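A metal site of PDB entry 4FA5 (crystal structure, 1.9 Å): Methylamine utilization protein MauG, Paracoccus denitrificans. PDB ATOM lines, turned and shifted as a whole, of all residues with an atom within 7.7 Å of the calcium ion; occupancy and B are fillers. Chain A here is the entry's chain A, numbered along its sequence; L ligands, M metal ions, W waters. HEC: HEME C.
The calcium ion is bound by OD1 of Asn 66 (2.1 Å), O of Pro 277 (2.3 Å), O of Thr 275 (2.3 Å), water W4 (2.4 Å), water W1 (2.4 Å), water W2 (2.4 Å) and water W3 (2.5 Å).
Within 4 Å of the calcium ion: Asn 66, Thr 275 and Pro 277. Along chain A the residues within 4 Å of the calcium ion span positions 66 to 277.
The backbone carbonyl oxygen (O) of Leu 51 is in hydrogen-bond range of the side-chain amide nitrogen (ND2) of Asn 66, 3.2 Å away. ND2 of Asn 66 lies close to O of Ala 52 (3.1 Å). The backbone NH (N) of Asn 66 lies within hydrogen-bond range of the backbone carbonyl oxygen (O) of His 280, 2.8 Å away. O of Asn 66 is in hydrogen-bond range of NE1 of Trp 93 (2.9 Å).
Water W1 bridges OG1 of Thr 275 (2.7 Å) and O2A of the ligand (2.9 Å). Water W2 bridges ND2 of Asn 66 (2.9 Å) and O of Gly 276 (2.9 Å). Water W3 bridges O1A of the ligand (2.7 Å) and O of Met 279 (3.1 Å).
N of His 280 lies within hydrogen-bond range of O1D of the ligand (2.7 Å). ND1 of His 280 sits at hydrogen-bond distance from O2D of the ligand (2.8 Å). The backbone NH (N) of Met 279 sits at hydrogen-bond distance from an oxygen (O1A) of the ligand.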
ATOM      1  N   ARG A  39     -14.337   4.822  13.451  1.00  0.00           N
ATOM      2  CA  ARG A  39     -15.342   4.692  14.493  1.00  0.00           C
ATOM      3  C   ARG A  39     -14.810   4.917  15.918  1.00  0.00           C
ATOM      4  O   ARG A  39     -15.077   4.167  16.784  1.00  0.00           O
ATOM      5  CB  ARG A  39     -15.993   3.334  14.440  1.00  0.00           C
ATOM      6  CG  ARG A  39     -17.397   3.332  14.884  1.00  0.00           C
ATOM      7  CD  ARG A  39     -18.002   1.963  14.887  1.00  0.00           C
ATOM      8  NE  ARG A  39     -19.387   2.025  15.256  1.00  0.00           N
ATOM      9  CZ  ARG A  39     -19.857   1.720  16.448  1.00  0.00           C
ATOM     10  NH1 ARG A  39     -21.133   1.808  16.688  1.00  0.00           N
ATOM     11  NH2 ARG A  39     -19.054   1.328  17.388  1.00  0.00           N
ATOM     12  N   THR A  42     -13.244   1.710  17.502  1.00  0.00           N
ATOM     13  CA  THR A  42     -14.129   0.639  17.996  1.00  0.00           C
ATOM     14  C   THR A  42     -14.585  -0.108  16.773  1.00  0.00           C
ATOM     15  O   THR A  42     -14.280   0.319  15.665  1.00  0.00           O
ATOM     16  CB  THR A  42     -15.377   1.190  18.791  1.00  0.00           C
ATOM     17  OG1 THR A  42     -16.178   2.022  17.936  1.00  0.00           O
ATOM     18  CG2 THR A  42     -14.929   2.022  20.002  1.00  0.00           C
ATOM     19  N   ASP A  43     -15.380  -1.155  16.969  1.00  0.00           N
ATOM     20  CA  ASP A  43     -15.635  -2.169  15.933  1.00  0.00           C
ATOM     21  C   ASP A  43     -16.985  -1.955  15.252  1.00  0.00           C
ATOM     22  O   ASP A  43     -18.076  -2.151  15.891  1.00  0.00           O
ATOM     23  CB  ASP A  43     -15.484  -3.580  16.478  1.00  0.00           C
ATOM     24  CG  ASP A  43     -15.494  -4.676  15.364  1.00  0.00           C
ATOM     25  OD1 ASP A  43     -15.335  -5.893  15.664  1.00  0.00           O
ATOM     26  OD2 ASP A  43     -15.644  -4.312  14.172  1.00  0.00           O
ATOM     27  N   LEU A  51     -23.285  -5.451  17.548  1.00  0.00           N
ATOM     28  CA  LEU A  51     -21.989  -4.842  17.673  1.00  0.00           C
ATOM     29  C   LEU A  51     -21.474  -4.987  19.098  1.00  0.00           C
ATOM     30  O   LEU A  51     -20.518  -4.324  19.464  1.00  0.00           O
ATOM     31  CB  LEU A  51     -22.059  -3.365  17.250  1.00  0.00           C
ATOM     32  CG  LEU A  51     -21.790  -2.859  15.812  1.00  0.00           C
ATOM     33  CD1 LEU A  51     -21.904  -3.853  14.705  1.00  0.00           C
ATOM     34  CD2 LEU A  51     -22.686  -1.663  15.528  1.00  0.00           C
ATOM     35  N   ALA A  52     -22.111  -5.865  19.877  1.00  0.00           N
ATOM     36  CA  ALA A  52     -21.830  -5.965  21.298  1.00  0.00           C
ATOM     37  C   ALA A  52     -20.459  -6.555  21.582  1.00  0.00           C
ATOM     38  O   ALA A  52     -19.777  -6.074  22.454  1.00  0.00           O
ATOM     39  CB  ALA A  52     -22.918  -6.696  22.082  1.00  0.00           C
ATOM     40  N   ASN A  66     -17.295  -5.860  24.971  1.00  0.00           N
ATOM     41  CA  ASN A  66     -17.432  -4.881  23.892  1.00  0.00           C
ATOM     42  C   ASN A  66     -16.068  -4.255  23.658  1.00  0.00           C
ATOM     43  O   ASN A  66     -15.311  -3.947  24.629  1.00  0.00           O
ATOM     44  CB  ASN A  66     -18.445  -3.830  24.314  1.00  0.00           C
ATOM     45  CG  ASN A  66     -18.632  -2.731  23.297  1.00  0.00           C
ATOM     46  OD1 ASN A  66     -18.402  -1.523  23.634  1.00  0.00           O
ATOM     47  ND2 ASN A  66     -19.110  -3.108  22.061  1.00  0.00           N
ATOM     48  N   THR A  67     -15.698  -4.135  22.382  1.00  0.00           N
ATOM     49  CA  THR A  67     -14.461  -3.477  22.072  1.00  0.00           C
ATOM     50  C   THR A  67     -14.499  -1.983  22.451  1.00  0.00           C
ATOM     51  O   THR A  67     -15.307  -1.240  21.913  1.00  0.00           O
ATOM     52  CB  THR A  67     -14.178  -3.642  20.587  1.00  0.00           C
ATOM     53  OG1 THR A  67     -13.999  -5.035  20.311  1.00  0.00           O
ATOM     54  CG2 THR A  67     -12.924  -2.835  20.218  1.00  0.00           C
ATOM     55  N   PRO A  68     -13.646  -1.548  23.382  1.00  0.00           N
ATOM     56  CA  PRO A  68     -13.637  -0.151  23.765  1.00  0.00           C
ATOM     57  C   PRO A  68     -12.795   0.714  22.793  1.00  0.00           C
ATOM     58  O   PRO A  68     -11.814   0.244  22.161  1.00  0.00           O
ATOM     59  CB  PRO A  68     -12.945  -0.169  25.177  1.00  0.00           C
ATOM     60  CG  PRO A  68     -11.994  -1.293  25.069  1.00  0.00           C
ATOM     61  CD  PRO A  68     -12.572  -2.308  24.069  1.00  0.00           C
ATOM     62  N   THR A  69     -13.096   2.003  22.760  1.00  0.00           N
ATOM     63  CA  THR A  69     -12.209   2.984  22.142  1.00  0.00           C
ATOM     64  C   THR A  69     -10.787   2.943  22.710  1.00  0.00           C
ATOM     65  O   THR A  69     -10.554   2.733  23.908  1.00  0.00           O
ATOM     66  CB  THR A  69     -12.771   4.376  22.306  1.00  0.00           C
ATOM     67  OG1 THR A  69     -11.995   5.289  21.535  1.00  0.00           O
ATOM     68  CG2 THR A  69     -12.745   4.799  23.834  1.00  0.00           C
ATOM     69  N   TRP A  93     -11.392  -3.858  30.399  1.00  0.00           N
ATOM     70  CA  TRP A  93     -12.498  -3.530  31.285  1.00  0.00           C
ATOM     71  C   TRP A  93     -12.294  -4.014  32.695  1.00  0.00           C
ATOM     72  O   TRP A  93     -12.875  -3.476  33.653  1.00  0.00           O
ATOM     73  CB  TRP A  93     -13.714  -4.182  30.689  1.00  0.00           C
ATOM     74  CG  TRP A  93     -14.264  -3.550  29.472  1.00  0.00           C
ATOM     75  CD1 TRP A  93     -14.134  -3.987  28.180  1.00  0.00           C
ATOM     76  CD2 TRP A  93     -15.132  -2.425  29.427  1.00  0.00           C
ATOM     77  NE1 TRP A  93     -14.860  -3.196  27.345  1.00  0.00           N
ATOM     78  CE2 TRP A  93     -15.500  -2.236  28.075  1.00  0.00           C
ATOM     79  CE3 TRP A  93     -15.683  -1.572  30.418  1.00  0.00           C
ATOM     80  CZ2 TRP A  93     -16.365  -1.210  27.667  1.00  0.00           C
ATOM     81  CZ3 TRP A  93     -16.529  -0.522  29.993  1.00  0.00           C
ATOM     82  CH2 TRP A  93     -16.884  -0.367  28.645  1.00  0.00           C
ATOM     83  N   VAL A 272     -18.202   8.863  23.738  1.00  0.00           N
ATOM     84  CA  VAL A 272     -19.194   7.870  24.147  1.00  0.00           C
ATOM     85  C   VAL A 272     -20.357   7.902  23.130  1.00  0.00           C
ATOM     86  O   VAL A 272     -20.984   6.860  22.853  1.00  0.00           O
ATOM     87  CB  VAL A 272     -19.711   8.028  25.628  1.00  0.00           C
ATOM     88  CG1 VAL A 272     -20.521   9.327  25.883  1.00  0.00           C
ATOM     89  CG2 VAL A 272     -20.485   6.799  26.084  1.00  0.00           C
ATOM     90  N   VAL A 274     -20.432   8.008  20.076  1.00  0.00           N
ATOM     91  CA  VAL A 274     -20.246   7.328  18.812  1.00  0.00           C
ATOM     92  C   VAL A 274     -19.629   5.937  18.998  1.00  0.00           C
ATOM     93  O   VAL A 274     -19.212   5.308  17.992  1.00  0.00           O
ATOM     94  CB  VAL A 274     -19.394   8.188  17.788  1.00  0.00           C
ATOM     95  CG1 VAL A 274     -19.985   9.552  17.626  1.00  0.00           C
ATOM     96  CG2 VAL A 274     -17.940   8.309  18.244  1.00  0.00           C
ATOM     97  N   THR A 275     -19.562   5.453  20.248  1.00  0.00           N
ATOM     98  CA  THR A 275     -18.929   4.121  20.467  1.00  0.00           C
ATOM     99  C   THR A 275     -19.907   3.099  21.024  1.00  0.00           C
ATOM    100  O   THR A 275     -19.519   2.167  21.685  1.00  0.00           O
ATOM    101  CB  THR A 275     -17.718   4.184  21.359  1.00  0.00           C
ATOM    102  OG1 THR A 275     -18.145   4.743  22.604  1.00  0.00           O
ATOM    103  CG2 THR A 275     -16.650   5.063  20.747  1.00  0.00           C
ATOM    104  N   GLY A 276     -21.202   3.264  20.763  1.00  0.00           N
ATOM    105  CA  GLY A 276     -22.184   2.213  21.083  1.00  0.00           C
ATOM    106  C   GLY A 276     -21.866   0.878  20.413  1.00  0.00           C
ATOM    107  O   GLY A 276     -21.104   0.829  19.425  1.00  0.00           O
ATOM    108  N   PRO A 277     -22.427  -0.220  20.951  1.00  0.00           N
ATOM    109  CA  PRO A 277     -23.257  -0.321  22.109  1.00  0.00           C
ATOM    110  C   PRO A 277     -22.437  -0.047  23.406  1.00  0.00           C
ATOM    111  O   PRO A 277     -21.207   0.114  23.323  1.00  0.00           O
ATOM    112  CB  PRO A 277     -23.775  -1.758  22.051  1.00  0.00           C
ATOM    113  CG  PRO A 277     -22.812  -2.460  21.217  1.00  0.00           C
ATOM    114  CD  PRO A 277     -22.146  -1.542  20.339  1.00  0.00           C
ATOM    115  N   TYR A 278     -23.117   0.007  24.565  1.00  0.00           N
ATOM    116  CA  TYR A 278     -22.454   0.448  25.808  1.00  0.00           C
ATOM    117  C   TYR A 278     -22.253  -0.612  26.874  1.00  0.00           C
ATOM    118  O   TYR A 278     -22.877  -1.676  26.833  1.00  0.00           O
ATOM    119  CB  TYR A 278     -23.193   1.646  26.373  1.00  0.00           C
ATOM    120  CG  TYR A 278     -23.206   2.707  25.343  1.00  0.00           C
ATOM    121  CD1 TYR A 278     -24.301   2.862  24.487  1.00  0.00           C
ATOM    122  CD2 TYR A 278     -22.085   3.516  25.130  1.00  0.00           C
ATOM    123  CE1 TYR A 278     -24.280   3.801  23.507  1.00  0.00           C
ATOM    124  CE2 TYR A 278     -22.085   4.462  24.182  1.00  0.00           C
ATOM    125  CZ  TYR A 278     -23.203   4.605  23.375  1.00  0.00           C
ATOM    126  OH  TYR A 278     -23.198   5.561  22.441  1.00  0.00           O
ATOM    127  N   MET A 279     -21.346  -0.306  27.808  1.00  0.00           N
ATOM    128  CA  MET A 279     -21.019  -1.126  28.973  1.00  0.00           C
ATOM    129  C   MET A 279     -20.086  -2.198  28.516  1.00  0.00           C
ATOM    130  O   MET A 279     -19.861  -2.377  27.287  1.00  0.00           O
ATOM    131  CB  MET A 279     -22.256  -1.702  29.723  1.00  0.00           C
ATOM    132  CG  MET A 279     -23.215  -0.613  30.172  1.00  0.00           C
ATOM    133  SD  MET A 279     -22.441   0.660  31.215  1.00  0.00           S
ATOM    134  CE  MET A 279     -23.853   1.783  31.415  1.00  0.00           C
ATOM    135  N   HIS A 280     -19.557  -2.928  29.476  1.00  0.00           N
ATOM    136  CA  HIS A 280     -18.484  -3.843  29.231  1.00  0.00           C
ATOM    137  C   HIS A 280     -18.864  -4.974  28.262  1.00  0.00           C
ATOM    138  O   HIS A 280     -17.987  -5.609  27.685  1.00  0.00           O
ATOM    139  CB  HIS A 280     -17.965  -4.398  30.556  1.00  0.00           C
ATOM    140  CG  HIS A 280     -18.950  -5.286  31.260  1.00  0.00           C
ATOM    141  ND1 HIS A 280     -19.610  -4.905  32.420  1.00  0.00           N
ATOM    142  CD2 HIS A 280     -19.375  -6.541  30.991  1.00  0.00           C
ATOM    143  CE1 HIS A 280     -20.421  -5.877  32.807  1.00  0.00           C
ATOM    144  NE2 HIS A 280     -20.289  -6.886  31.969  1.00  0.00           N
ATOM    145  N   ASN A 281     -20.162  -5.250  28.134  1.00  0.00           N
ATOM    146  CA  ASN A 281     -20.643  -6.365  27.352  1.00  0.00           C
ATOM    147  C   ASN A 281     -21.535  -5.894  26.229  1.00  0.00           C
ATOM    148  O   ASN A 281     -22.201  -6.712  25.587  1.00  0.00           O
ATOM    149  CB  ASN A 281     -21.411  -7.370  28.220  1.00  0.00           C
ATOM    150  CG  ASN A 281     -22.575  -6.707  29.007  1.00  0.00           C
ATOM    151  OD1 ASN A 281     -22.979  -5.577  28.725  1.00  0.00           O
ATOM    152  ND2 ASN A 281     -23.071  -7.398  29.991  1.00  0.00           N
ATOM    153  N   GLY A 282     -21.554  -4.588  26.010  1.00  0.00           N
ATOM    154  CA  GLY A 282     -22.309  -4.010  24.891  1.00  0.00           C
ATOM    155  C   GLY A 282     -23.803  -4.218  25.033  1.00  0.00           C
ATOM    156  O   GLY A 282     -24.520  -4.217  24.044  1.00  0.00           O
ATOM    157  N   PHE A 284     -26.326  -2.396  26.045  1.00  0.00           N
ATOM    158  CA  PHE A 284     -27.218  -1.344  25.578  1.00  0.00           C
ATOM    159  C   PHE A 284     -26.747  -0.712  24.289  1.00  0.00           C
ATOM    160  O   PHE A 284     -25.621  -0.189  24.216  1.00  0.00           O
ATOM    161  CB  PHE A 284     -27.366  -0.218  26.609  1.00  0.00           C
ATOM    162  CG  PHE A 284     -27.595  -0.695  28.018  1.00  0.00           C
ATOM    163  CD1 PHE A 284     -28.577  -1.654  28.317  1.00  0.00           C
ATOM    164  CD2 PHE A 284     -26.853  -0.151  29.060  1.00  0.00           C
ATOM    165  CE1 PHE A 284     -28.801  -2.074  29.633  1.00  0.00           C
ATOM    166  CE2 PHE A 284     -27.063  -0.564  30.394  1.00  0.00           C
ATOM    167  CZ  PHE A 284     -28.026  -1.549  30.675  1.00  0.00           C
HETATM  168 FE   HEC L   1     -21.355   5.541  34.504  1.00  0.00          FE
HETATM  169  CHA HEC L   1     -20.421   3.275  32.165  1.00  0.00           C
HETATM  170  CHB HEC L   1     -22.683   7.493  32.108  1.00  0.00           C
HETATM  171  CHC HEC L   1     -22.966   7.349  36.971  1.00  0.00           C
HETATM  172  CHD HEC L   1     -19.350   4.187  36.837  1.00  0.00           C
HETATM  173  NA  HEC L   1     -21.522   5.394  32.437  1.00  0.00           N
HETATM  174  C1A HEC L   1     -21.121   4.414  31.632  1.00  0.00           C
HETATM  175  C2A HEC L   1     -21.481   4.547  30.213  1.00  0.00           C
HETATM  176  C3A HEC L   1     -22.157   5.754  30.188  1.00  0.00           C
HETATM  177  C4A HEC L   1     -22.137   6.206  31.610  1.00  0.00           C
HETATM  178  CMA HEC L   1     -22.784   6.450  29.016  1.00  0.00           C
HETATM  179  CAA HEC L   1     -21.124   3.567  29.114  1.00  0.00           C
HETATM  180  CBA HEC L   1     -19.773   4.090  28.593  1.00  0.00           C
HETATM  181  CGA HEC L   1     -19.154   3.054  27.650  1.00  0.00           C
HETATM  182  O1A HEC L   1     -19.681   1.899  27.583  1.00  0.00           O
HETATM  183  O2A HEC L   1     -18.120   3.368  26.973  1.00  0.00           O
HETATM  184  NB  HEC L   1     -22.633   7.118  34.531  1.00  0.00           N
HETATM  185  C1B HEC L   1     -23.014   7.823  33.490  1.00  0.00           C
HETATM  186  C2B HEC L   1     -23.850   8.998  33.828  1.00  0.00           C
HETATM  187  C3B HEC L   1     -23.944   8.939  35.194  1.00  0.00           C
HETATM  188  C4B HEC L   1     -23.149   7.766  35.578  1.00  0.00           C
HETATM  189  CMB HEC L   1     -24.417   9.954  32.805  1.00  0.00           C
HETATM  190  CAB HEC L   1     -24.693   9.854  36.117  1.00  0.00           C
HETATM  191  CBB HEC L   1     -26.117   9.523  35.812  1.00  0.00           C
HETATM  192  NC  HEC L   1     -21.185   5.720  36.577  1.00  0.00           N
HETATM  193  C1C HEC L   1     -21.922   6.462  37.402  1.00  0.00           C
HETATM  194  C2C HEC L   1     -21.548   6.335  38.805  1.00  0.00           C
HETATM  195  C3C HEC L   1     -20.492   5.425  38.801  1.00  0.00           C
HETATM  196  C4C HEC L   1     -20.346   5.093  37.362  1.00  0.00           C
HETATM  197  CMC HEC L   1     -22.194   7.055  39.958  1.00  0.00           C
HETATM  198  CAC HEC L   1     -19.651   4.896  39.940  1.00  0.00           C
HETATM  199  CBC HEC L   1     -20.537   4.265  40.988  1.00  0.00           C
HETATM  200  ND  HEC L   1     -20.077   3.987  34.484  1.00  0.00           N
HETATM  201  C1D HEC L   1     -19.407   3.492  35.542  1.00  0.00           C
HETATM  202  C2D HEC L   1     -18.720   2.236  35.247  1.00  0.00           C
HETATM  203  C3D HEC L   1     -19.036   2.006  33.901  1.00  0.00           C
HETATM  204  C4D HEC L   1     -19.871   3.127  33.503  1.00  0.00           C
HETATM  205  CMD HEC L   1     -17.927   1.365  36.118  1.00  0.00           C
HETATM  206  CAD HEC L   1     -18.715   0.809  33.081  1.00  0.00           C
HETATM  207  CBD HEC L   1     -19.749  -0.164  33.664  1.00  0.00           C
HETATM  208  CGD HEC L   1     -19.575  -1.558  33.108  1.00  0.00           C
HETATM  209  O1D HEC L   1     -19.550  -1.744  31.861  1.00  0.00           O
HETATM  210  O2D HEC L   1     -19.442  -2.497  33.885  1.00  0.00           O
HETATM  211 CA    CA M   1     -18.932   0.500  23.229  1.00  0.00          CA
HETATM  212  O   HOH W   1     -18.699   2.670  24.175  1.00  0.00           O
HETATM  213  O   HOH W   2     -19.004  -0.419  20.998  1.00  0.00           O
HETATM  214  O   HOH W   3     -18.850   0.117  25.674  1.00  0.00           O
HETATM  215  O   HOH W   4     -16.694   1.002  22.676  1.00  0.00           O
